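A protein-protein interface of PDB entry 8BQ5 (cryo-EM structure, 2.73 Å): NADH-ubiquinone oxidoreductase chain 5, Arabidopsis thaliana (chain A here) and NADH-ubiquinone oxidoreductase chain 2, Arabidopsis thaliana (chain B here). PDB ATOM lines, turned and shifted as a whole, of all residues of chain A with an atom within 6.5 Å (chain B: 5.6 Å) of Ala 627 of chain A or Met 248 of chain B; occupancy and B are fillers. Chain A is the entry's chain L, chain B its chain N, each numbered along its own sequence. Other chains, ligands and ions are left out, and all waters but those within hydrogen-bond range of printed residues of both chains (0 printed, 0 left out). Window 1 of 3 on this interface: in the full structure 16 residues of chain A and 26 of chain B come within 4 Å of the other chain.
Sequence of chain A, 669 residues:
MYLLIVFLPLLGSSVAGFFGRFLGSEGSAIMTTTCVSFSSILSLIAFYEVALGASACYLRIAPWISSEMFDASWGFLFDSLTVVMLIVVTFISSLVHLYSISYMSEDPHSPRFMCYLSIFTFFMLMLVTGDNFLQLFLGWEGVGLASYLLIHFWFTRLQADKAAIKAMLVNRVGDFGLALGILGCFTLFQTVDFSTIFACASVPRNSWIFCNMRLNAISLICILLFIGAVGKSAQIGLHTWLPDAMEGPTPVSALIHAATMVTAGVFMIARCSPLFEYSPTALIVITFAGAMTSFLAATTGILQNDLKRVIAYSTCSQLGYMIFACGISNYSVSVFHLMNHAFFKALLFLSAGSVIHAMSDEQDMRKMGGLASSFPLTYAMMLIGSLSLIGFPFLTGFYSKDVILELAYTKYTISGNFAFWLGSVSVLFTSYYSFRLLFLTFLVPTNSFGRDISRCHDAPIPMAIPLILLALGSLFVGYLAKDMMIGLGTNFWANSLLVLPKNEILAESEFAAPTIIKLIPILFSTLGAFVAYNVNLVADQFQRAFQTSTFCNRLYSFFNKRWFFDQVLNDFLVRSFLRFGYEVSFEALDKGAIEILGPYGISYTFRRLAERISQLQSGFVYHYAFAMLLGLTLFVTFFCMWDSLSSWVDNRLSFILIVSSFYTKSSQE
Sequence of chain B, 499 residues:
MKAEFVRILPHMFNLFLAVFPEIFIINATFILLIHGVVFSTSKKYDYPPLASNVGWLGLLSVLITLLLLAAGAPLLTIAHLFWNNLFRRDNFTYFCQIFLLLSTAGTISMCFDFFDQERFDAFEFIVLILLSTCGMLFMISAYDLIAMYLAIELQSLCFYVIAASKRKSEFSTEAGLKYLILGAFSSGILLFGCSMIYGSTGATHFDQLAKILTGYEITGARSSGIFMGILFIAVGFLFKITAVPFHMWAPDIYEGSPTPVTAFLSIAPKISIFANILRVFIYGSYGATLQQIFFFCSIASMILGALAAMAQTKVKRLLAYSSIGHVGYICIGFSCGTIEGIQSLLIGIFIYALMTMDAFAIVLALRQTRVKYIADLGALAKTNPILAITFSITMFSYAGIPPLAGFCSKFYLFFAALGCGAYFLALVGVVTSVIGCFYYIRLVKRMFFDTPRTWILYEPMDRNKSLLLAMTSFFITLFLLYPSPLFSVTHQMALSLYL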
ATOM      1  N   LEU A 616      -7.086   6.645   9.882  1.00  0.00           N
ATOM      2  CA  LEU A 616      -7.605   7.798   9.154  1.00  0.00           C
ATOM      3  C   LEU A 616      -8.987   8.183   9.658  1.00  0.00           C
ATOM      4  O   LEU A 616      -9.291   9.370   9.817  1.00  0.00           O
ATOM      5  CB  LEU A 616      -7.651   7.504   7.657  1.00  0.00           C
ATOM      6  CG  LEU A 616      -6.592   8.231   6.842  1.00  0.00           C
ATOM      7  CD1 LEU A 616      -6.898   9.711   6.844  1.00  0.00           C
ATOM      8  CD2 LEU A 616      -5.221   7.957   7.422  1.00  0.00           C
ATOM      9  N   GLN A 617      -9.836   7.191   9.916  1.00  0.00           N
ATOM     10  CA  GLN A 617     -11.113   7.431  10.568  1.00  0.00           C
ATOM     11  C   GLN A 617     -10.843   7.737  12.034  1.00  0.00           C
ATOM     12  O   GLN A 617     -10.967   6.861  12.894  1.00  0.00           O
ATOM     13  CB  GLN A 617     -12.033   6.220  10.414  1.00  0.00           C
ATOM     14  CG  GLN A 617     -13.483   6.485  10.764  1.00  0.00           C
ATOM     15  CD  GLN A 617     -14.238   7.170   9.644  1.00  0.00           C
ATOM     16  OE1 GLN A 617     -13.738   7.295   8.527  1.00  0.00           O
ATOM     17  NE2 GLN A 617     -15.451   7.618   9.938  1.00  0.00           N
ATOM     18  N   SER A 618     -10.459   8.979  12.317  1.00  0.00           N
ATOM     19  CA  SER A 618      -9.928   9.331  13.626  1.00  0.00           C
ATOM     20  C   SER A 618     -11.008   9.548  14.673  1.00  0.00           C
ATOM     21  O   SER A 618     -10.696   9.576  15.867  1.00  0.00           O
ATOM     22  CB  SER A 618      -9.074  10.595  13.515  1.00  0.00           C
ATOM     23  OG  SER A 618      -9.806  11.635  12.895  1.00  0.00           O
ATOM     24  N   TYR A 622     -13.685  17.307  12.680  1.00  0.00           N
ATOM     25  CA  TYR A 622     -12.861  18.248  11.930  1.00  0.00           C
ATOM     26  C   TYR A 622     -12.092  17.546  10.819  1.00  0.00           C
ATOM     27  O   TYR A 622     -11.952  18.086   9.716  1.00  0.00           O
ATOM     28  CB  TYR A 622     -11.891  18.965  12.864  1.00  0.00           C
ATOM     29  CG  TYR A 622     -10.920  19.860  12.135  1.00  0.00           C
ATOM     30  CD1 TYR A 622     -11.335  21.074  11.602  1.00  0.00           C
ATOM     31  CD2 TYR A 622      -9.592  19.491  11.970  1.00  0.00           C
ATOM     32  CE1 TYR A 622     -10.451  21.899  10.939  1.00  0.00           C
ATOM     33  CE2 TYR A 622      -8.703  20.308  11.303  1.00  0.00           C
ATOM     34  CZ  TYR A 622      -9.139  21.511  10.789  1.00  0.00           C
ATOM     35  OH  TYR A 622      -8.258  22.331  10.125  1.00  0.00           O
ATOM     36  N   HIS A 623     -11.576  16.347  11.099  1.00  0.00           N
ATOM     37  CA  HIS A 623     -10.811  15.616  10.095  1.00  0.00           C
ATOM     38  C   HIS A 623     -11.672  15.260   8.891  1.00  0.00           C
ATOM     39  O   HIS A 623     -11.211  15.330   7.748  1.00  0.00           O
ATOM     40  CB  HIS A 623     -10.206  14.357  10.713  1.00  0.00           C
ATOM     41  CG  HIS A 623      -8.896  14.591  11.398  1.00  0.00           C
ATOM     42  ND1 HIS A 623      -8.485  13.854  12.487  1.00  0.00           N
ATOM     43  CD2 HIS A 623      -7.907  15.481  11.151  1.00  0.00           C
ATOM     44  CE1 HIS A 623      -7.298  14.281  12.882  1.00  0.00           C
ATOM     45  NE2 HIS A 623      -6.925  15.266  12.087  1.00  0.00           N
ATOM     46  N   TYR A 624     -12.931  14.881   9.124  1.00  0.00           N
ATOM     47  CA  TYR A 624     -13.805  14.501   8.016  1.00  0.00           C
ATOM     48  C   TYR A 624     -14.151  15.703   7.143  1.00  0.00           C
ATOM     49  O   TYR A 624     -14.132  15.610   5.909  1.00  0.00           O
ATOM     50  CB  TYR A 624     -15.080  13.843   8.549  1.00  0.00           C
ATOM     51  CG  TYR A 624     -14.853  12.688   9.506  1.00  0.00           C
ATOM     52  CD1 TYR A 624     -13.630  12.032   9.567  1.00  0.00           C
ATOM     53  CD2 TYR A 624     -15.867  12.253  10.347  1.00  0.00           C
ATOM     54  CE1 TYR A 624     -13.423  10.985  10.439  1.00  0.00           C
ATOM     55  CE2 TYR A 624     -15.669  11.204  11.221  1.00  0.00           C
ATOM     56  CZ  TYR A 624     -14.444  10.573  11.261  1.00  0.00           C
ATOM     57  OH  TYR A 624     -14.234   9.526  12.126  1.00  0.00           O
ATOM     58  N   ALA A 625     -14.470  16.839   7.766  1.00  0.00           N
ATOM     59  CA  ALA A 625     -14.731  18.053   6.999  1.00  0.00           C
ATOM     60  C   ALA A 625     -13.492  18.487   6.228  1.00  0.00           C
ATOM     61  O   ALA A 625     -13.589  18.920   5.074  1.00  0.00           O
ATOM     62  CB  ALA A 625     -15.207  19.168   7.928  1.00  0.00           C
ATOM     63  N   PHE A 626     -12.320  18.374   6.856  1.00  0.00           N
ATOM     64  CA  PHE A 626     -11.067  18.691   6.182  1.00  0.00           C
ATOM     65  C   PHE A 626     -10.834  17.768   4.994  1.00  0.00           C
ATOM     66  O   PHE A 626     -10.323  18.198   3.957  1.00  0.00           O
ATOM     67  CB  PHE A 626      -9.917  18.595   7.185  1.00  0.00           C
ATOM     68  CG  PHE A 626      -8.603  19.094   6.663  1.00  0.00           C
ATOM     69  CD1 PHE A 626      -8.536  20.237   5.887  1.00  0.00           C
ATOM     70  CD2 PHE A 626      -7.428  18.437   6.981  1.00  0.00           C
ATOM     71  CE1 PHE A 626      -7.324  20.701   5.420  1.00  0.00           C
ATOM     72  CE2 PHE A 626      -6.213  18.897   6.516  1.00  0.00           C
ATOM     73  CZ  PHE A 626      -6.161  20.030   5.735  1.00  0.00           C
ATOM     74  N   ALA A 627     -11.200  16.492   5.130  1.00  0.00           N
ATOM     75  CA  ALA A 627     -11.104  15.568   4.007  1.00  0.00           C
ATOM     76  C   ALA A 627     -12.026  15.983   2.868  1.00  0.00           C
ATOM     77  O   ALA A 627     -11.629  15.950   1.699  1.00  0.00           O
ATOM     78  CB  ALA A 627     -11.424  14.146   4.466  1.00  0.00           C
ATOM     79  N   MET A 628     -13.262  16.374   3.186  1.00  0.00           N
ATOM     80  CA  MET A 628     -14.176  16.833   2.138  1.00  0.00           C
ATOM     81  C   MET A 628     -13.627  18.067   1.430  1.00  0.00           C
ATOM     82  O   MET A 628     -13.670  18.163   0.195  1.00  0.00           O
ATOM     83  CB  MET A 628     -15.554  17.130   2.729  1.00  0.00           C
ATOM     84  CG  MET A 628     -16.115  16.022   3.597  1.00  0.00           C
ATOM     85  SD  MET A 628     -17.889  16.138   3.890  1.00  0.00           S
ATOM     86  CE  MET A 628     -18.401  17.181   2.530  1.00  0.00           C
ATOM     87  N   LEU A 629     -13.109  19.022   2.202  1.00  0.00           N
ATOM     88  CA  LEU A 629     -12.551  20.240   1.623  1.00  0.00           C
ATOM     89  C   LEU A 629     -11.337  19.934   0.752  1.00  0.00           C
ATOM     90  O   LEU A 629     -11.190  20.493  -0.342  1.00  0.00           O
ATOM     91  CB  LEU A 629     -12.184  21.214   2.739  1.00  0.00           C
ATOM     92  CG  LEU A 629     -11.557  22.551   2.357  1.00  0.00           C
ATOM     93  CD1 LEU A 629     -12.321  23.214   1.221  1.00  0.00           C
ATOM     94  CD2 LEU A 629     -11.508  23.448   3.576  1.00  0.00           C
ATOM     95  N   LEU A 630     -10.458  19.047   1.222  1.00  0.00           N
ATOM     96  CA  LEU A 630      -9.283  18.676   0.443  1.00  0.00           C
ATOM     97  C   LEU A 630      -9.674  17.930  -0.824  1.00  0.00           C
ATOM     98  O   LEU A 630      -9.029  18.082  -1.865  1.00  0.00           O
ATOM     99  CB  LEU A 630      -8.338  17.829   1.292  1.00  0.00           C
ATOM    100  CG  LEU A 630      -7.387  18.573   2.227  1.00  0.00           C
ATOM    101  CD1 LEU A 630      -6.553  17.579   3.013  1.00  0.00           C
ATOM    102  CD2 LEU A 630      -6.493  19.519   1.442  1.00  0.00           C
ATOM    103  N   GLY A 631     -10.726  17.112  -0.756  1.00  0.00           N
ATOM    104  CA  GLY A 631     -11.195  16.430  -1.950  1.00  0.00           C
ATOM    105  C   GLY A 631     -11.749  17.389  -2.983  1.00  0.00           C
ATOM    106  O   GLY A 631     -11.472  17.260  -4.178  1.00  0.00           O
ATOM    107  N   LEU A 632     -12.533  18.373  -2.535  1.00  0.00           N
ATOM    108  CA  LEU A 632     -13.018  19.406  -3.447  1.00  0.00           C
ATOM    109  C   LEU A 632     -11.861  20.187  -4.066  1.00  0.00           C
ATOM    110  O   LEU A 632     -11.860  20.464  -5.275  1.00  0.00           O
ATOM    111  CB  LEU A 632     -13.968  20.344  -2.705  1.00  0.00           C
ATOM    112  CG  LEU A 632     -14.564  21.531  -3.465  1.00  0.00           C
ATOM    113  CD1 LEU A 632     -15.510  21.073  -4.561  1.00  0.00           C
ATOM    114  CD2 LEU A 632     -15.269  22.468  -2.498  1.00  0.00           C
ATOM    115  N   LEU B 182     -21.623  17.443   8.527  1.00  0.00           N
ATOM    116  CA  LEU B 182     -21.044  17.089   7.234  1.00  0.00           C
ATOM    117  C   LEU B 182     -22.089  17.125   6.121  1.00  0.00           C
ATOM    118  O   LEU B 182     -21.789  17.540   4.992  1.00  0.00           O
ATOM    119  CB  LEU B 182     -20.368  15.722   7.322  1.00  0.00           C
ATOM    120  CG  LEU B 182     -19.257  15.655   8.376  1.00  0.00           C
ATOM    121  CD1 LEU B 182     -18.808  14.230   8.626  1.00  0.00           C
ATOM    122  CD2 LEU B 182     -18.075  16.519   7.966  1.00  0.00           C
ATOM    123  N   PRO B 245     -13.273  10.456  -1.682  1.00  0.00           N
ATOM    124  CA  PRO B 245     -12.941  10.819  -0.297  1.00  0.00           C
ATOM    125  C   PRO B 245     -14.033  11.565   0.454  1.00  0.00           C
ATOM    126  O   PRO B 245     -13.743  12.290   1.400  1.00  0.00           O
ATOM    127  CB  PRO B 245     -11.710  11.710  -0.481  1.00  0.00           C
ATOM    128  CG  PRO B 245     -11.920  12.383  -1.823  1.00  0.00           C
ATOM    129  CD  PRO B 245     -12.907  11.540  -2.609  1.00  0.00           C
ATOM    130  N   PHE B 246     -15.298  11.414   0.071  1.00  0.00           N
ATOM    131  CA  PHE B 246     -16.413  12.063   0.757  1.00  0.00           C
ATOM    132  C   PHE B 246     -17.234  11.048   1.540  1.00  0.00           C
ATOM    133  O   PHE B 246     -18.467  11.083   1.554  1.00  0.00           O
ATOM    134  CB  PHE B 246     -17.267  12.831  -0.243  1.00  0.00           C
ATOM    135  CG  PHE B 246     -16.460  13.647  -1.212  1.00  0.00           C
ATOM    136  CD1 PHE B 246     -15.970  14.889  -0.848  1.00  0.00           C
ATOM    137  CD2 PHE B 246     -16.184  13.171  -2.483  1.00  0.00           C
ATOM    138  CE1 PHE B 246     -15.221  15.642  -1.730  1.00  0.00           C
ATOM    139  CE2 PHE B 246     -15.437  13.923  -3.372  1.00  0.00           C
ATOM    140  CZ  PHE B 246     -14.956  15.159  -2.994  1.00  0.00           C
ATOM    141  N   HIS B 247     -16.535  10.133   2.208  1.00  0.00           N
ATOM    142  CA  HIS B 247     -17.102   8.912   2.762  1.00  0.00           C
ATOM    143  C   HIS B 247     -17.020   8.802   4.276  1.00  0.00           C
ATOM    144  O   HIS B 247     -17.779   8.026   4.857  1.00  0.00           O
ATOM    145  CB  HIS B 247     -16.380   7.701   2.165  1.00  0.00           C
ATOM    146  CG  HIS B 247     -14.991   7.529   2.691  1.00  0.00           C
ATOM    147  ND1 HIS B 247     -13.940   8.317   2.276  1.00  0.00           N
ATOM    148  CD2 HIS B 247     -14.486   6.690   3.625  1.00  0.00           C
ATOM    149  CE1 HIS B 247     -12.843   7.960   2.920  1.00  0.00           C
ATOM    150  NE2 HIS B 247     -13.147   6.974   3.744  1.00  0.00           N
ATOM    151  N   MET B 248     -16.118   9.540   4.933  1.00  0.00           N
ATOM    152  CA  MET B 248     -15.784   9.228   6.322  1.00  0.00           C
ATOM    153  C   MET B 248     -16.965   9.380   7.272  1.00  0.00           C
ATOM    154  O   MET B 248     -16.943   8.799   8.361  1.00  0.00           O
ATOM    155  CB  MET B 248     -14.620  10.090   6.817  1.00  0.00           C
ATOM    156  CG  MET B 248     -13.576  10.418   5.773  1.00  0.00           C
ATOM    157  SD  MET B 248     -12.030  11.024   6.467  1.00  0.00           S
ATOM    158  CE  MET B 248     -11.713   9.785   7.717  1.00  0.00           C
ATOM    159  N   TRP B 249     -17.991  10.144   6.897  1.00  0.00           N
ATOM    160  CA  TRP B 249     -19.179  10.237   7.741  1.00  0.00           C
ATOM    161  C   TRP B 249     -19.872   8.887   7.868  1.00  0.00           C
ATOM    162  O   TRP B 249     -20.376   8.538   8.942  1.00  0.00           O
ATOM    163  CB  TRP B 249     -20.146  11.278   7.179  1.00  0.00           C
ATOM    164  CG  TRP B 249     -20.793  10.873   5.890  1.00  0.00           C
ATOM    165  CD1 TRP B 249     -20.287  11.035   4.636  1.00  0.00           C
ATOM    166  CD2 TRP B 249     -22.064  10.233   5.729  1.00  0.00           C
ATOM    167  NE1 TRP B 249     -21.164  10.543   3.703  1.00  0.00           N
ATOM    168  CE2 TRP B 249     -22.264  10.043   4.348  1.00  0.00           C
ATOM    169  CE3 TRP B 249     -23.054   9.803   6.618  1.00  0.00           C
ATOM    170  CZ2 TRP B 249     -23.411   9.444   3.836  1.00  0.00           C
ATOM    171  CZ3 TRP B 249     -24.191   9.206   6.108  1.00  0.00           C
ATOM    172  CH2 TRP B 249     -24.360   9.033   4.729  1.00  0.00           C
ATOM    173  N   ALA B 250     -19.897   8.113   6.784  1.00  0.00           N
ATOM    174  CA  ALA B 250     -20.755   6.931   6.723  1.00  0.00           C
ATOM    175  C   ALA B 250     -20.423   5.870   7.767  1.00  0.00           C
ATOM    176  O   ALA B 250     -21.360   5.367   8.407  1.00  0.00           O
ATOM    177  CB  ALA B 250     -20.721   6.350   5.307  1.00  0.00           C
ATOM    178  N   PRO B 251     -19.167   5.457   7.980  1.00  0.00           N
ATOM    179  CA  PRO B 251     -18.940   4.425   9.010  1.00  0.00           C
ATOM    180  C   PRO B 251     -19.347   4.865  10.408  1.00  0.00           C
ATOM    181  O   PRO B 251     -20.008   4.098  11.125  1.00  0.00           O
ATOM    182  CB  PRO B 251     -17.433   4.137   8.903  1.00  0.00           C
ATOM    183  CG  PRO B 251     -17.004   4.708   7.602  1.00  0.00           C
ATOM    184  CD  PRO B 251     -17.913   5.849   7.315  1.00  0.00           C
ATOM    185  N   ASP B 252     -18.999   6.093  10.806  1.00  0.00           N
ATOM    186  CA  ASP B 252     -19.370   6.583  12.131  1.00  0.00           C
ATOM    187  C   ASP B 252     -20.880   6.692  12.294  1.00  0.00           C
ATOM    188  O   ASP B 252     -21.428   6.286  13.325  1.00  0.00           O
ATOM    189  CB  ASP B 252     -18.719   7.940  12.395  1.00  0.00           C
ATOM    190  CG  ASP B 252     -17.250   7.828  12.732  1.00  0.00           C
ATOM    191  OD1 ASP B 252     -16.737   8.726  13.433  1.00  0.00           O
ATOM    192  OD2 ASP B 252     -16.610   6.848  12.305  1.00  0.00           O
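The side-chain hydroxyl of Tyr 624 of chain A lies within hydrogen-bond range of the side-chain amide nitrogen of Gln 617 of chain A (3.1 Å). O of Phe 246 of chain B sits at hydrogen-bond distance from NE1 of Trp 249 of chain B.
Printed residues of chain A that touch a printed residue of chain B: Leu 616, Gln 617, Tyr 624, Ala 625, Ala 627, Met 628, Gly 631 and Leu 632. Along chain A the printed residues that touch a printed residue of chain B span positions 616 to 632. Among the printed residues, 11 pairs touch across the chains.
Tyr 622 of chain A touches none of the printed residues of chain B. Of the printed residues of chain B, Tyr 624 of chain A touches Leu 182, Met 248 and Asp 252. Phe 626 of chain A touches none of the printed residues of chain B. Printed residues of chain B within 4 Å of Ala 627 of chain A: Met 248 (3.8 Å). Printed residues of chain B within 4 Å of Met 628 of chain A: Phe 246. Of the printed residues of chain B, Leu 632 of chain A touches Phe 246. Printed residues of chain A within 4 Å of Phe 246 of chain B: Met 628, Gly 631 and Leu 632. The nearest residue of chain B that does not touch Ala 627 of chain A is Pro 245 of chain B (4.2 Å). The nearest printed residue of chain B that does not touch Leu 616 of chain A is His 247 of chain B (6.8 Å).
Met 248 of chain B touches Leu 616 of chain A. CB of Tyr 624 of chain A touches CD1 of Leu 182 of chain B, 3.7 Å away. Met 248 of chain B touches Tyr 624 of chain A. CD2 of Leu 182 of chain B touches N of Ala 625 of chain A, 3.6 Å away. SD of Met 248 of chain B touches CB of Ala 627 of chain A (3.8 Å). Phe 246 of chain B touches Met 628 of chain A. Phe 246 of chain B touches Gly 631 of chain A (CZ to C, 3.9 Å). N of Leu 632 of chain A touches CE1 of Phe 246 of chain B, 3.9 Å away.
O of Met 248 of chain B sits at hydrogen-bond distance from NE2 of Gln 617 of chain A (2.5 Å). The side-chain amide nitrogen of Gln 617 of chain A lies within hydrogen-bond range of the side-chain carboxylate of Asp 252 of chain B. The side-chain hydroxyl (OH) of Tyr 624 of chain A lies within hydrogen-bond range of the side-chain carboxylate (OD1) of Asp 252 of chain B, at 2.9 Å.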
